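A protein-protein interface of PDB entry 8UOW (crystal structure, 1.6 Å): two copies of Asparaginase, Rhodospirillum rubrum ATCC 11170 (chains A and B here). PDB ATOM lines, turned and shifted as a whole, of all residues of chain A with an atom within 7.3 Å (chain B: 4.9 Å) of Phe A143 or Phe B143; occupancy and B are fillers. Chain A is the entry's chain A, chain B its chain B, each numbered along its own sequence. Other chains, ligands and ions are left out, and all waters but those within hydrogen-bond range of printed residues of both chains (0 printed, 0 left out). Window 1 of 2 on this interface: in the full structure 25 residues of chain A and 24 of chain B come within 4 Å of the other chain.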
ATOM      1  N   LEU A  21      26.276  11.261  -7.415  1.00  0.00           N
ATOM      2  CA  LEU A  21      25.972  10.902  -6.008  1.00  0.00           C
ATOM      3  C   LEU A  21      26.079  12.137  -5.116  1.00  0.00           C
ATOM      4  O   LEU A  21      27.110  12.859  -5.168  1.00  0.00           O
ATOM      5  CB  LEU A  21      26.980   9.841  -5.573  1.00  0.00           C
ATOM      6  CG  LEU A  21      26.890   9.389  -4.131  1.00  0.00           C
ATOM      7  CD1 LEU A  21      25.603   8.646  -3.791  1.00  0.00           C
ATOM      8  CD2 LEU A  21      28.080   8.524  -3.809  1.00  0.00           C
ATOM      9  N   LEU A  57      38.841   9.897  -6.659  1.00  0.00           N
ATOM     10  CA  LEU A  57      37.617   9.827  -7.465  1.00  0.00           C
ATOM     11  C   LEU A  57      37.865  10.390  -8.880  1.00  0.00           C
ATOM     12  O   LEU A  57      38.501  11.445  -8.994  1.00  0.00           O
ATOM     13  CB  LEU A  57      36.524  10.611  -6.771  1.00  0.00           C
ATOM     14  CG  LEU A  57      36.107  10.104  -5.392  1.00  0.00           C
ATOM     15  CD1 LEU A  57      35.099  11.045  -4.759  1.00  0.00           C
ATOM     16  CD2 LEU A  57      35.594   8.682  -5.474  1.00  0.00           C
ATOM     17  N   LEU A  95      23.430   8.876  -0.618  1.00  0.00           N
ATOM     18  CA  LEU A  95      23.940   8.101   0.552  1.00  0.00           C
ATOM     19  C   LEU A  95      23.808   8.956   1.808  1.00  0.00           C
ATOM     20  O   LEU A  95      24.205  10.124   1.758  1.00  0.00           O
ATOM     21  CB  LEU A  95      25.415   7.764   0.333  1.00  0.00           C
ATOM     22  CG  LEU A  95      26.124   7.164   1.546  1.00  0.00           C
ATOM     23  CD1 LEU A  95      25.501   5.871   2.028  1.00  0.00           C
ATOM     24  CD2 LEU A  95      27.585   6.918   1.201  1.00  0.00           C
ATOM     25  N   VAL A 122      20.477   5.143  -0.032  1.00  0.00           N
ATOM     26  CA  VAL A 122      21.152   4.160   0.826  1.00  0.00           C
ATOM     27  C   VAL A 122      21.584   4.792   2.131  1.00  0.00           C
ATOM     28  O   VAL A 122      22.102   5.866   2.112  1.00  0.00           O
ATOM     29  CB  VAL A 122      22.344   3.548   0.084  1.00  0.00           C
ATOM     30  CG1 VAL A 122      23.082   2.541   0.925  1.00  0.00           C
ATOM     31  CG2 VAL A 122      21.851   2.868  -1.196  1.00  0.00           C
ATOM     32  N   SER A 124      23.930   4.140   5.561  1.00  0.00           N
ATOM     33  CA  SER A 124      25.051   3.313   6.053  1.00  0.00           C
ATOM     34  C   SER A 124      25.714   4.059   7.196  1.00  0.00           C
ATOM     35  O   SER A 124      25.322   5.164   7.545  1.00  0.00           O
ATOM     36  CB  SER A 124      26.058   2.998   4.936  1.00  0.00           C
ATOM     37  OG  SER A 124      26.943   1.974   5.346  1.00  0.00           O
ATOM     38  N   ALA A 137      34.299   1.303   8.729  1.00  0.00           N
ATOM     39  CA  ALA A 137      33.775   2.519   8.062  1.00  0.00           C
ATOM     40  C   ALA A 137      34.212   2.627   6.583  1.00  0.00           C
ATOM     41  O   ALA A 137      33.324   2.838   5.711  1.00  0.00           O
ATOM     42  CB  ALA A 137      34.189   3.771   8.795  1.00  0.00           C
ATOM     43  N   ALA A 138      35.489   2.525   6.273  1.00  0.00           N
ATOM     44  CA  ALA A 138      35.940   2.825   4.901  1.00  0.00           C
ATOM     45  C   ALA A 138      35.353   1.803   3.900  1.00  0.00           C
ATOM     46  O   ALA A 138      34.796   2.154   2.841  1.00  0.00           O
ATOM     47  CB  ALA A 138      37.441   2.871   4.802  1.00  0.00           C
ATOM     48  N   PHE A 139      35.399   0.517   4.262  1.00  0.00           N
ATOM     49  CA  PHE A 139      34.734  -0.565   3.479  1.00  0.00           C
ATOM     50  C   PHE A 139      33.261  -0.218   3.261  1.00  0.00           C
ATOM     51  O   PHE A 139      32.691  -0.296   2.159  1.00  0.00           O
ATOM     52  CB  PHE A 139      34.898  -1.922   4.142  1.00  0.00           C
ATOM     53  CG  PHE A 139      34.153  -3.030   3.433  1.00  0.00           C
ATOM     54  CD1 PHE A 139      32.824  -3.302   3.681  1.00  0.00           C
ATOM     55  CD2 PHE A 139      34.759  -3.684   2.380  1.00  0.00           C
ATOM     56  CE1 PHE A 139      32.130  -4.251   2.957  1.00  0.00           C
ATOM     57  CE2 PHE A 139      34.081  -4.667   1.686  1.00  0.00           C
ATOM     58  CZ  PHE A 139      32.799  -4.969   1.996  1.00  0.00           C
ATOM     59  N   ASN A 140      32.570   0.099   4.357  1.00  0.00           N
ATOM     60  CA  ASN A 140      31.109   0.337   4.295  1.00  0.00           C
ATOM     61  C   ASN A 140      30.819   1.525   3.399  1.00  0.00           C
ATOM     62  O   ASN A 140      29.809   1.511   2.695  1.00  0.00           O
ATOM     63  CB  ASN A 140      30.546   0.624   5.680  1.00  0.00           C
ATOM     64  CG  ASN A 140      30.563  -0.529   6.644  1.00  0.00           C
ATOM     65  OD1 ASN A 140      30.692  -1.689   6.266  1.00  0.00           O
ATOM     66  ND2 ASN A 140      30.314  -0.205   7.901  1.00  0.00           N
ATOM     67  N   ILE A 141      31.642   2.568   3.433  1.00  0.00           N
ATOM     68  CA  ILE A 141      31.425   3.765   2.593  1.00  0.00           C
ATOM     69  C   ILE A 141      31.601   3.366   1.127  1.00  0.00           C
ATOM     70  O   ILE A 141      30.792   3.716   0.330  1.00  0.00           O
ATOM     71  CB  ILE A 141      32.340   4.908   3.034  1.00  0.00           C
ATOM     72  CG1 ILE A 141      31.846   5.487   4.360  1.00  0.00           C
ATOM     73  CG2 ILE A 141      32.448   5.973   1.964  1.00  0.00           C
ATOM     74  CD1 ILE A 141      32.869   6.261   5.110  1.00  0.00           C
ATOM     75  N   GLY A 142      32.663   2.649   0.787  1.00  0.00           N
ATOM     76  CA  GLY A 142      32.812   2.220  -0.614  1.00  0.00           C
ATOM     77  C   GLY A 142      31.668   1.355  -1.069  1.00  0.00           C
ATOM     78  O   GLY A 142      31.133   1.551  -2.144  1.00  0.00           O
ATOM     79  N   PHE A 143      31.260   0.402  -0.253  1.00  0.00           N
ATOM     80  CA  PHE A 143      30.153  -0.501  -0.570  1.00  0.00           C
ATOM     81  C   PHE A 143      28.866   0.294  -0.747  1.00  0.00           C
ATOM     82  O   PHE A 143      28.127   0.066  -1.715  1.00  0.00           O
ATOM     83  CB  PHE A 143      30.022  -1.584   0.490  1.00  0.00           C
ATOM     84  CG  PHE A 143      29.091  -2.701   0.130  1.00  0.00           C
ATOM     85  CD1 PHE A 143      27.744  -2.557   0.426  1.00  0.00           C
ATOM     86  CD2 PHE A 143      29.560  -3.885  -0.402  1.00  0.00           C
ATOM     87  CE1 PHE A 143      26.852  -3.572   0.050  1.00  0.00           C
ATOM     88  CE2 PHE A 143      28.663  -4.892  -0.773  1.00  0.00           C
ATOM     89  CZ  PHE A 143      27.324  -4.734  -0.508  1.00  0.00           C
ATOM     90  N   ALA A 144      28.605   1.251   0.139  1.00  0.00           N
ATOM     91  CA  ALA A 144      27.344   2.012   0.112  1.00  0.00           C
ATOM     92  C   ALA A 144      27.304   2.976  -1.069  1.00  0.00           C
ATOM     93  O   ALA A 144      26.214   3.233  -1.595  1.00  0.00           O
ATOM     94  CB  ALA A 144      27.117   2.682   1.431  1.00  0.00           C
ATOM     95  N   CYS A 145      28.429   3.562  -1.401  1.00  0.00           N
ATOM     96  CA  CYS A 145      28.536   4.469  -2.564  1.00  0.00           C
ATOM     97  C   CYS A 145      28.128   3.655  -3.798  1.00  0.00           C
ATOM     98  O   CYS A 145      27.376   4.122  -4.649  1.00  0.00           O
ATOM     99  CB  CYS A 145      29.927   5.078  -2.699  1.00  0.00           C
ATOM    100  SG  CYS A 145      30.262   6.444  -1.550  1.00  0.00           S
ATOM    101  N   ALA A 146      28.740   2.510  -3.980  1.00  0.00           N
ATOM    102  CA  ALA A 146      28.430   1.689  -5.159  1.00  0.00           C
ATOM    103  C   ALA A 146      26.962   1.294  -5.091  1.00  0.00           C
ATOM    104  O   ALA A 146      26.272   1.413  -6.139  1.00  0.00           O
ATOM    105  CB  ALA A 146      29.321   0.483  -5.178  1.00  0.00           C
ATOM    106  N   ALA A 147      26.432   0.914  -3.930  1.00  0.00           N
ATOM    107  CA  ALA A 147      25.019   0.494  -3.819  1.00  0.00           C
ATOM    108  C   ALA A 147      24.113   1.665  -4.230  1.00  0.00           C
ATOM    109  O   ALA A 147      23.137   1.452  -5.000  1.00  0.00           O
ATOM    110  CB  ALA A 147      24.694  -0.037  -2.461  1.00  0.00           C
ATOM    111  N   ALA A 148      24.444   2.891  -3.807  1.00  0.00           N
ATOM    112  CA  ALA A 148      23.616   4.081  -4.119  1.00  0.00           C
ATOM    113  C   ALA A 148      23.596   4.304  -5.644  1.00  0.00           C
ATOM    114  O   ALA A 148      22.576   4.797  -6.202  1.00  0.00           O
ATOM    115  CB  ALA A 148      24.114   5.297  -3.373  1.00  0.00           C
ATOM    116  N   LEU A 149      24.702   4.043  -6.330  1.00  0.00           N
ATOM    117  CA  LEU A 149      24.812   4.184  -7.811  1.00  0.00           C
ATOM    118  C   LEU A 149      24.107   3.054  -8.553  1.00  0.00           C
ATOM    119  O   LEU A 149      23.602   3.319  -9.675  1.00  0.00           O
ATOM    120  CB  LEU A 149      26.273   4.314  -8.208  1.00  0.00           C
ATOM    121  CG  LEU A 149      26.969   5.575  -7.699  1.00  0.00           C
ATOM    122  CD1 LEU A 149      28.470   5.443  -7.856  1.00  0.00           C
ATOM    123  CD2 LEU A 149      26.473   6.798  -8.456  1.00  0.00           C
ATOM    124  N   MET A 150      24.099   1.834  -8.031  1.00  0.00           N
ATOM    125  CA  MET A 150      23.796   0.637  -8.858  1.00  0.00           C
ATOM    126  C   MET A 150      22.417   0.064  -8.536  1.00  0.00           C
ATOM    127  O   MET A 150      21.834  -0.587  -9.431  1.00  0.00           O
ATOM    128  CB  MET A 150      24.856  -0.435  -8.672  1.00  0.00           C
ATOM    129  CG  MET A 150      26.182   0.040  -9.138  1.00  0.00           C
ATOM    130  SD  MET A 150      27.529  -1.103  -8.631  1.00  0.00           S
ATOM    131  CE  MET A 150      28.901  -0.039  -9.067  1.00  0.00           C
ATOM    132  N   LEU A 151      21.859   0.271  -7.356  1.00  0.00           N
ATOM    133  CA  LEU A 151      20.541  -0.331  -7.002  1.00  0.00           C
ATOM    134  C   LEU A 151      19.433   0.440  -7.716  1.00  0.00           C
ATOM    135  O   LEU A 151      19.561   1.658  -7.938  1.00  0.00           O
ATOM    136  CB  LEU A 151      20.328  -0.303  -5.489  1.00  0.00           C
ATOM    137  CG  LEU A 151      21.193  -1.268  -4.697  1.00  0.00           C
ATOM    138  CD1 LEU A 151      21.087  -0.973  -3.229  1.00  0.00           C
ATOM    139  CD2 LEU A 151      20.788  -2.693  -5.009  1.00  0.00           C
ATOM    140  N   ILE A 157      19.353  -0.200   3.433  1.00  0.00           N
ATOM    141  CA  ILE A 157      20.498  -0.149   4.395  1.00  0.00           C
ATOM    142  C   ILE A 157      21.613  -1.035   3.805  1.00  0.00           C
ATOM    143  O   ILE A 157      21.390  -2.200   3.464  1.00  0.00           O
ATOM    144  CB  ILE A 157      20.059  -0.596   5.800  1.00  0.00           C
ATOM    145  CG1 ILE A 157      19.195   0.508   6.415  1.00  0.00           C
ATOM    146  CG2 ILE A 157      21.231  -1.016   6.665  1.00  0.00           C
ATOM    147  CD1 ILE A 157      18.396   0.088   7.622  1.00  0.00           C
ATOM    148  N   ALA A 158      22.814  -0.467   3.670  1.00  0.00           N
ATOM    149  CA  ALA A 158      23.995  -1.207   3.186  1.00  0.00           C
ATOM    150  C   ALA A 158      24.942  -1.342   4.375  1.00  0.00           C
ATOM    151  O   ALA A 158      25.546  -0.326   4.798  1.00  0.00           O
ATOM    152  CB  ALA A 158      24.673  -0.518   2.021  1.00  0.00           C
ATOM    153  N   MET A 159      25.096  -2.565   4.853  1.00  0.00           N
ATOM    154  CA  MET A 159      26.003  -2.899   5.981  1.00  0.00           C
ATOM    155  C   MET A 159      26.455  -4.360   5.842  1.00  0.00           C
ATOM    156  O   MET A 159      25.721  -5.137   5.243  1.00  0.00           O
ATOM    157  CB  MET A 159      25.332  -2.634   7.341  1.00  0.00           C
ATOM    158  CG  MET A 159      25.017  -1.183   7.641  1.00  0.00           C
ATOM    159  SD  MET A 159      26.487  -0.139   7.987  1.00  0.00           S
ATOM    160  CE  MET A 159      26.839  -0.669   9.657  1.00  0.00           C
ATOM    161  N   HIS A 160      27.586  -4.718   6.436  1.00  0.00           N
ATOM    162  CA  HIS A 160      28.031  -6.133   6.477  1.00  0.00           C
ATOM    163  C   HIS A 160      28.190  -6.713   5.068  1.00  0.00           C
ATOM    164  O   HIS A 160      28.054  -7.917   4.827  1.00  0.00           O
ATOM    165  CB  HIS A 160      27.017  -7.037   7.233  1.00  0.00           C
ATOM    166  CG  HIS A 160      26.603  -6.403   8.521  1.00  0.00           C
ATOM    167  ND1 HIS A 160      27.507  -6.122   9.525  1.00  0.00           N
ATOM    168  CD2 HIS A 160      25.383  -5.987   8.969  1.00  0.00           C
ATOM    169  CE1 HIS A 160      26.853  -5.579  10.552  1.00  0.00           C
ATOM    170  NE2 HIS A 160      25.576  -5.416  10.204  1.00  0.00           N
ATOM    171  N   GLY A 161      28.519  -5.866   4.095  1.00  0.00           N
ATOM    172  CA  GLY A 161      28.687  -6.309   2.701  1.00  0.00           C
ATOM    173  C   GLY A 161      27.413  -6.841   2.072  1.00  0.00           C
ATOM    174  O   GLY A 161      27.459  -7.639   1.139  1.00  0.00           O
ATOM    175  N   LYS A 162      26.279  -6.327   2.491  1.00  0.00           N
ATOM    176  CA  LYS A 162      24.995  -6.689   1.851  1.00  0.00           C
ATOM    177  C   LYS A 162      23.973  -5.577   1.962  1.00  0.00           C
ATOM    178  O   LYS A 162      24.202  -4.534   2.634  1.00  0.00           O
ATOM    179  CB  LYS A 162      24.433  -7.980   2.429  1.00  0.00           C
ATOM    180  CG  LYS A 162      24.039  -7.882   3.859  1.00  0.00           C
ATOM    181  CD  LYS A 162      23.222  -9.126   4.328  1.00  0.00           C
ATOM    182  CE  LYS A 162      21.785  -8.980   3.900  1.00  0.00           C
ATOM    183  NZ  LYS A 162      20.958 -10.135   4.305  1.00  0.00           N
ATOM    184  N   VAL A 163      22.881  -5.791   1.218  1.00  0.00           N
ATOM    185  CA  VAL A 163      21.768  -4.828   1.100  1.00  0.00           C
ATOM    186  C   VAL A 163      20.587  -5.346   1.904  1.00  0.00           C
ATOM    187  O   VAL A 163      20.181  -6.485   1.661  1.00  0.00           O
ATOM    188  CB  VAL A 163      21.397  -4.582  -0.365  1.00  0.00           C
ATOM    189  CG1 VAL A 163      20.305  -3.542  -0.500  1.00  0.00           C
ATOM    190  CG2 VAL A 163      22.619  -4.091  -1.088  1.00  0.00           C
ATOM    191  N   PHE B 139      38.365   1.733   0.463  1.00  0.00           N
ATOM    192  CA  PHE B 139      37.198   2.255  -0.261  1.00  0.00           C
ATOM    193  C   PHE B 139      37.004   1.425  -1.546  1.00  0.00           C
ATOM    194  O   PHE B 139      35.953   0.982  -1.923  1.00  0.00           O
ATOM    195  CB  PHE B 139      37.387   3.750  -0.583  1.00  0.00           C
ATOM    196  CG  PHE B 139      36.320   4.288  -1.500  1.00  0.00           C
ATOM    197  CD1 PHE B 139      36.484   4.222  -2.881  1.00  0.00           C
ATOM    198  CD2 PHE B 139      35.166   4.869  -1.001  1.00  0.00           C
ATOM    199  CE1 PHE B 139      35.504   4.682  -3.727  1.00  0.00           C
ATOM    200  CE2 PHE B 139      34.189   5.337  -1.852  1.00  0.00           C
ATOM    201  CZ  PHE B 139      34.359   5.232  -3.197  1.00  0.00           C
ATOM    202  N   ASN B 140      38.109   1.198  -2.247  1.00  0.00           N
ATOM    203  CA  ASN B 140      38.062   0.534  -3.574  1.00  0.00           C
ATOM    204  C   ASN B 140      37.538  -0.887  -3.359  1.00  0.00           C
ATOM    205  O   ASN B 140      36.775  -1.377  -4.193  1.00  0.00           O
ATOM    206  CB  ASN B 140      39.441   0.474  -4.226  1.00  0.00           C
ATOM    207  CG  ASN B 140      39.908   1.792  -4.799  1.00  0.00           C
ATOM    208  OD1 ASN B 140      39.136   2.766  -4.849  1.00  0.00           O
ATOM    209  ND2 ASN B 140      41.170   1.830  -5.193  1.00  0.00           N
ATOM    210  N   ILE B 141      37.992  -1.556  -2.319  1.00  0.00           N
ATOM    211  CA  ILE B 141      37.531  -2.941  -2.030  1.00  0.00           C
ATOM    212  C   ILE B 141      36.022  -2.945  -1.738  1.00  0.00           C
ATOM    213  O   ILE B 141      35.286  -3.768  -2.299  1.00  0.00           O
ATOM    214  CB  ILE B 141      38.355  -3.507  -0.869  1.00  0.00           C
ATOM    215  CG1 ILE B 141      39.790  -3.812  -1.301  1.00  0.00           C
ATOM    216  CG2 ILE B 141      37.685  -4.728  -0.261  1.00  0.00           C
ATOM    217  CD1 ILE B 141      40.699  -4.029  -0.153  1.00  0.00           C
ATOM    218  N   GLY B 142      35.534  -2.052  -0.904  1.00  0.00           N
ATOM    219  CA  GLY B 142      34.086  -1.971  -0.649  1.00  0.00           C
ATOM    220  C   GLY B 142      33.300  -1.736  -1.930  1.00  0.00           C
ATOM    221  O   GLY B 142      32.279  -2.378  -2.215  1.00  0.00           O
ATOM    222  N   PHE B 143      33.732  -0.749  -2.715  1.00  0.00           N
ATOM    223  CA  PHE B 143      33.037  -0.355  -3.960  1.00  0.00           C
ATOM    224  C   PHE B 143      33.021  -1.553  -4.910  1.00  0.00           C
ATOM    225  O   PHE B 143      32.002  -1.818  -5.479  1.00  0.00           O
ATOM    226  CB  PHE B 143      33.728   0.923  -4.488  1.00  0.00           C
ATOM    227  CG  PHE B 143      33.007   1.553  -5.643  1.00  0.00           C
ATOM    228  CD1 PHE B 143      33.127   1.034  -6.939  1.00  0.00           C
ATOM    229  CD2 PHE B 143      32.171   2.640  -5.450  1.00  0.00           C
ATOM    230  CE1 PHE B 143      32.411   1.604  -8.002  1.00  0.00           C
ATOM    231  CE2 PHE B 143      31.466   3.201  -6.508  1.00  0.00           C
ATOM    232  CZ  PHE B 143      31.603   2.694  -7.784  1.00  0.00           C
ATOM    233  N   ALA B 144      34.140  -2.223  -5.017  1.00  0.00           N
ATOM    234  CA  ALA B 144      34.347  -3.346  -5.975  1.00  0.00           C
ATOM    235  C   ALA B 144      33.509  -4.544  -5.535  1.00  0.00           C
ATOM    236  O   ALA B 144      33.021  -5.277  -6.417  1.00  0.00           O
ATOM    237  CB  ALA B 144      35.809  -3.651  -6.174  1.00  0.00           C
ATOM    238  N   CYS B 145      33.455  -4.831  -4.253  1.00  0.00           N
ATOM    239  CA  CYS B 145      32.604  -5.923  -3.709  1.00  0.00           C
ATOM    240  C   CYS B 145      31.160  -5.672  -4.074  1.00  0.00           C
ATOM    241  O   CYS B 145      30.500  -6.599  -4.634  1.00  0.00           O
ATOM    242  CB  CYS B 145      32.779  -6.135  -2.214  1.00  0.00           C
ATOM    243  SG  CYS B 145      34.340  -6.908  -1.738  1.00  0.00           S
ATOM    244  N   ALA B 146      30.643  -4.477  -3.853  1.00  0.00           N
ATOM    245  CA  ALA B 146      29.262  -4.153  -4.249  1.00  0.00           C
ATOM    246  C   ALA B 146      29.095  -4.326  -5.756  1.00  0.00           C
ATOM    247  O   ALA B 146      28.073  -4.859  -6.216  1.00  0.00           O
ATOM    248  CB  ALA B 146      28.965  -2.753  -3.841  1.00  0.00           C
ATOM    249  N   ALA B 147      30.027  -3.801  -6.552  1.00  0.00           N
ATOM    250  CA  ALA B 147      29.906  -3.893  -8.009  1.00  0.00           C
ATOM    251  C   ALA B 147      29.837  -5.373  -8.378  1.00  0.00           C
ATOM    252  O   ALA B 147      29.009  -5.680  -9.268  1.00  0.00           O
ATOM    253  CB  ALA B 147      31.025  -3.143  -8.637  1.00  0.00           C
ATOM    254  N   LEU B 149      28.716  -7.840  -6.852  1.00  0.00           N
ATOM    255  CA  LEU B 149      27.386  -8.390  -6.460  1.00  0.00           C
ATOM    256  C   LEU B 149      26.227  -7.794  -7.279  1.00  0.00           C
ATOM    257  O   LEU B 149      25.202  -8.515  -7.431  1.00  0.00           O
ATOM    258  CB  LEU B 149      27.167  -8.141  -4.968  1.00  0.00           C
ATOM    259  CG  LEU B 149      28.101  -8.923  -4.038  1.00  0.00           C
ATOM    260  CD1 LEU B 149      27.877  -8.432  -2.627  1.00  0.00           C
ATOM    261  CD2 LEU B 149      27.893 -10.440  -4.102  1.00  0.00           C
ATOM    262  N   MET B 150      26.323  -6.542  -7.766  1.00  0.00           N
ATOM    263  CA  MET B 150      25.159  -5.802  -8.304  1.00  0.00           C
ATOM    264  C   MET B 150      25.181  -5.662  -9.813  1.00  0.00           C
ATOM    265  O   MET B 150      24.088  -5.382 -10.375  1.00  0.00           O
ATOM    266  CB  MET B 150      25.100  -4.421  -7.670  1.00  0.00           C
ATOM    267  CG  MET B 150      24.859  -4.577  -6.208  1.00  0.00           C
ATOM    268  SD  MET B 150      25.001  -2.973  -5.377  1.00  0.00           S
ATOM    269  CE  MET B 150      25.146  -3.520  -3.684  1.00  0.00           C
ATOM    270  N   ALA B 158      36.599  -1.566 -11.539  1.00  0.00           N
ATOM    271  CA  ALA B 158      35.998  -0.616 -10.583  1.00  0.00           C
ATOM    272  C   ALA B 158      37.109   0.129  -9.860  1.00  0.00           C
ATOM    273  O   ALA B 158      37.841  -0.454  -9.030  1.00  0.00           O
ATOM    274  CB  ALA B 158      35.140  -1.375  -9.599  1.00  0.00           C
ATOM    275  N   GLY B 161      35.818   5.282  -7.794  1.00  0.00           N
ATOM    276  CA  GLY B 161      34.386   5.356  -7.527  1.00  0.00           C
ATOM    277  C   GLY B 161      33.512   5.299  -8.763  1.00  0.00           C
ATOM    278  O   GLY B 161      32.369   5.844  -8.722  1.00  0.00           O
ATOM    279  N   LYS B 162      33.952   4.600  -9.795  1.00  0.00           N
ATOM    280  CA  LYS B 162      33.110   4.353 -10.983  1.00  0.00           C
ATOM    281  C   LYS B 162      33.482   3.028 -11.615  1.00  0.00           C
ATOM    282  O   LYS B 162      34.452   2.376 -11.217  1.00  0.00           O
ATOM    283  CB  LYS B 162      33.222   5.529 -11.939  1.00  0.00           C
ATOM    284  CG  LYS B 162      34.604   5.679 -12.515  1.00  0.00           C
ATOM    285  CD  LYS B 162      34.596   6.660 -13.681  1.00  0.00           C
ATOM    286  CE  LYS B 162      34.113   5.952 -14.914  1.00  0.00           C
ATOM    287  NZ  LYS B 162      34.288   6.749 -16.144  1.00  0.00           N
ATOM    288  N   VAL B 163      32.664   2.659 -12.580  1.00  0.00           N
ATOM    289  CA  VAL B 163      32.790   1.364 -13.298  1.00  0.00           C
ATOM    290  C   VAL B 163      33.246   1.674 -14.721  1.00  0.00           C
ATOM    291  O   VAL B 163      32.583   2.505 -15.407  1.00  0.00           O
ATOM    292  CB  VAL B 163      31.443   0.642 -13.288  1.00  0.00           C
ATOM    293  CG1 VAL B 163      31.508  -0.649 -14.089  1.00  0.00           C
ATOM    294  CG2 VAL B 163      31.029   0.376 -11.856  1.00  0.00           C
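Phe A139 touches Gly B142, and with the chains exchanged Gly A142 touches Phe B139. Phe A143 touches Ala B146, and with the chains exchanged Ala A146 touches Phe B143. Ala B146 touches its own counterpart, Ala A146. Leu A149 touches Phe B143, but with the chains exchanged Phe A143 does not touch Leu B149 (4.1 Å).
Phe A143 touches just these residues of chain B: Gly B142, Phe B143 and Ala B146. Of the printed residues of chain A, Phe B143 touches Gly A142, Phe A143, Ala A146 and Leu A149. Gly B142 touches three residues of chain A. Printed residues of chain B within 4 Å of Ala A146: Phe B143 (3.5 Å) and Ala B146 (3.5 Å). Of the printed residues of chain B, Ala A138 touches Phe B139 (3.9 Å). Printed residues of chain A within 4 Å of Leu B149: Gly A161. Lys B162 touches none of the printed residues of chain A. The nearest residue of chain B that does not touch Phe A143 is Met B150 (4.04 Å).
Of the 27 printed residues of chain A, 10 touch a printed residue of chain B. Hydrophobic or aromatic side chains of chain A within 4 Å of the printed part of chain B: Phe A139, Phe A143, Ala A146, Ala A147, Leu A149, Met A150 and Val A163. Of the 15 printed residues of chain B, 8 touch a printed residue of chain A. Among the printed residues, 16 pairs touch across the chains. Among the printed residues, no Asp or Glu carboxylate lies within 4 Å of a Lys or Arg side-chain nitrogen of the other chain.
Among the printed residues, pairs that only touch across the chains: Ala A138 with Phe B139 (3.9 Å), Phe A139 with Gly B142 (3.5 Å), Gly A142 with Phe B139 (3.6 Å), Gly A142 with Gly B142 (3.6 Å), Gly A142 with Phe B143 (3.2 Å), Phe A143 with Gly B142 (3.3 Å), Phe A143 with Phe B143 (3.7 Å), Phe A143 with Ala B146 (3.6 Å), Ala A146 with Phe B143 (3.5 Å), Ala A146 with Ala B146 (3.5 Å), Ala A147 with Met B150 (3.7 Å), Leu A149 with Phe B143 (3.98 Å), Met A150 with Ala B147 (3.7 Å), Met A150 with Val B163 (3.5 Å), Gly A161 with Leu B149 (3.9 Å) and Val A163 with Met B150 (3.7 Å).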
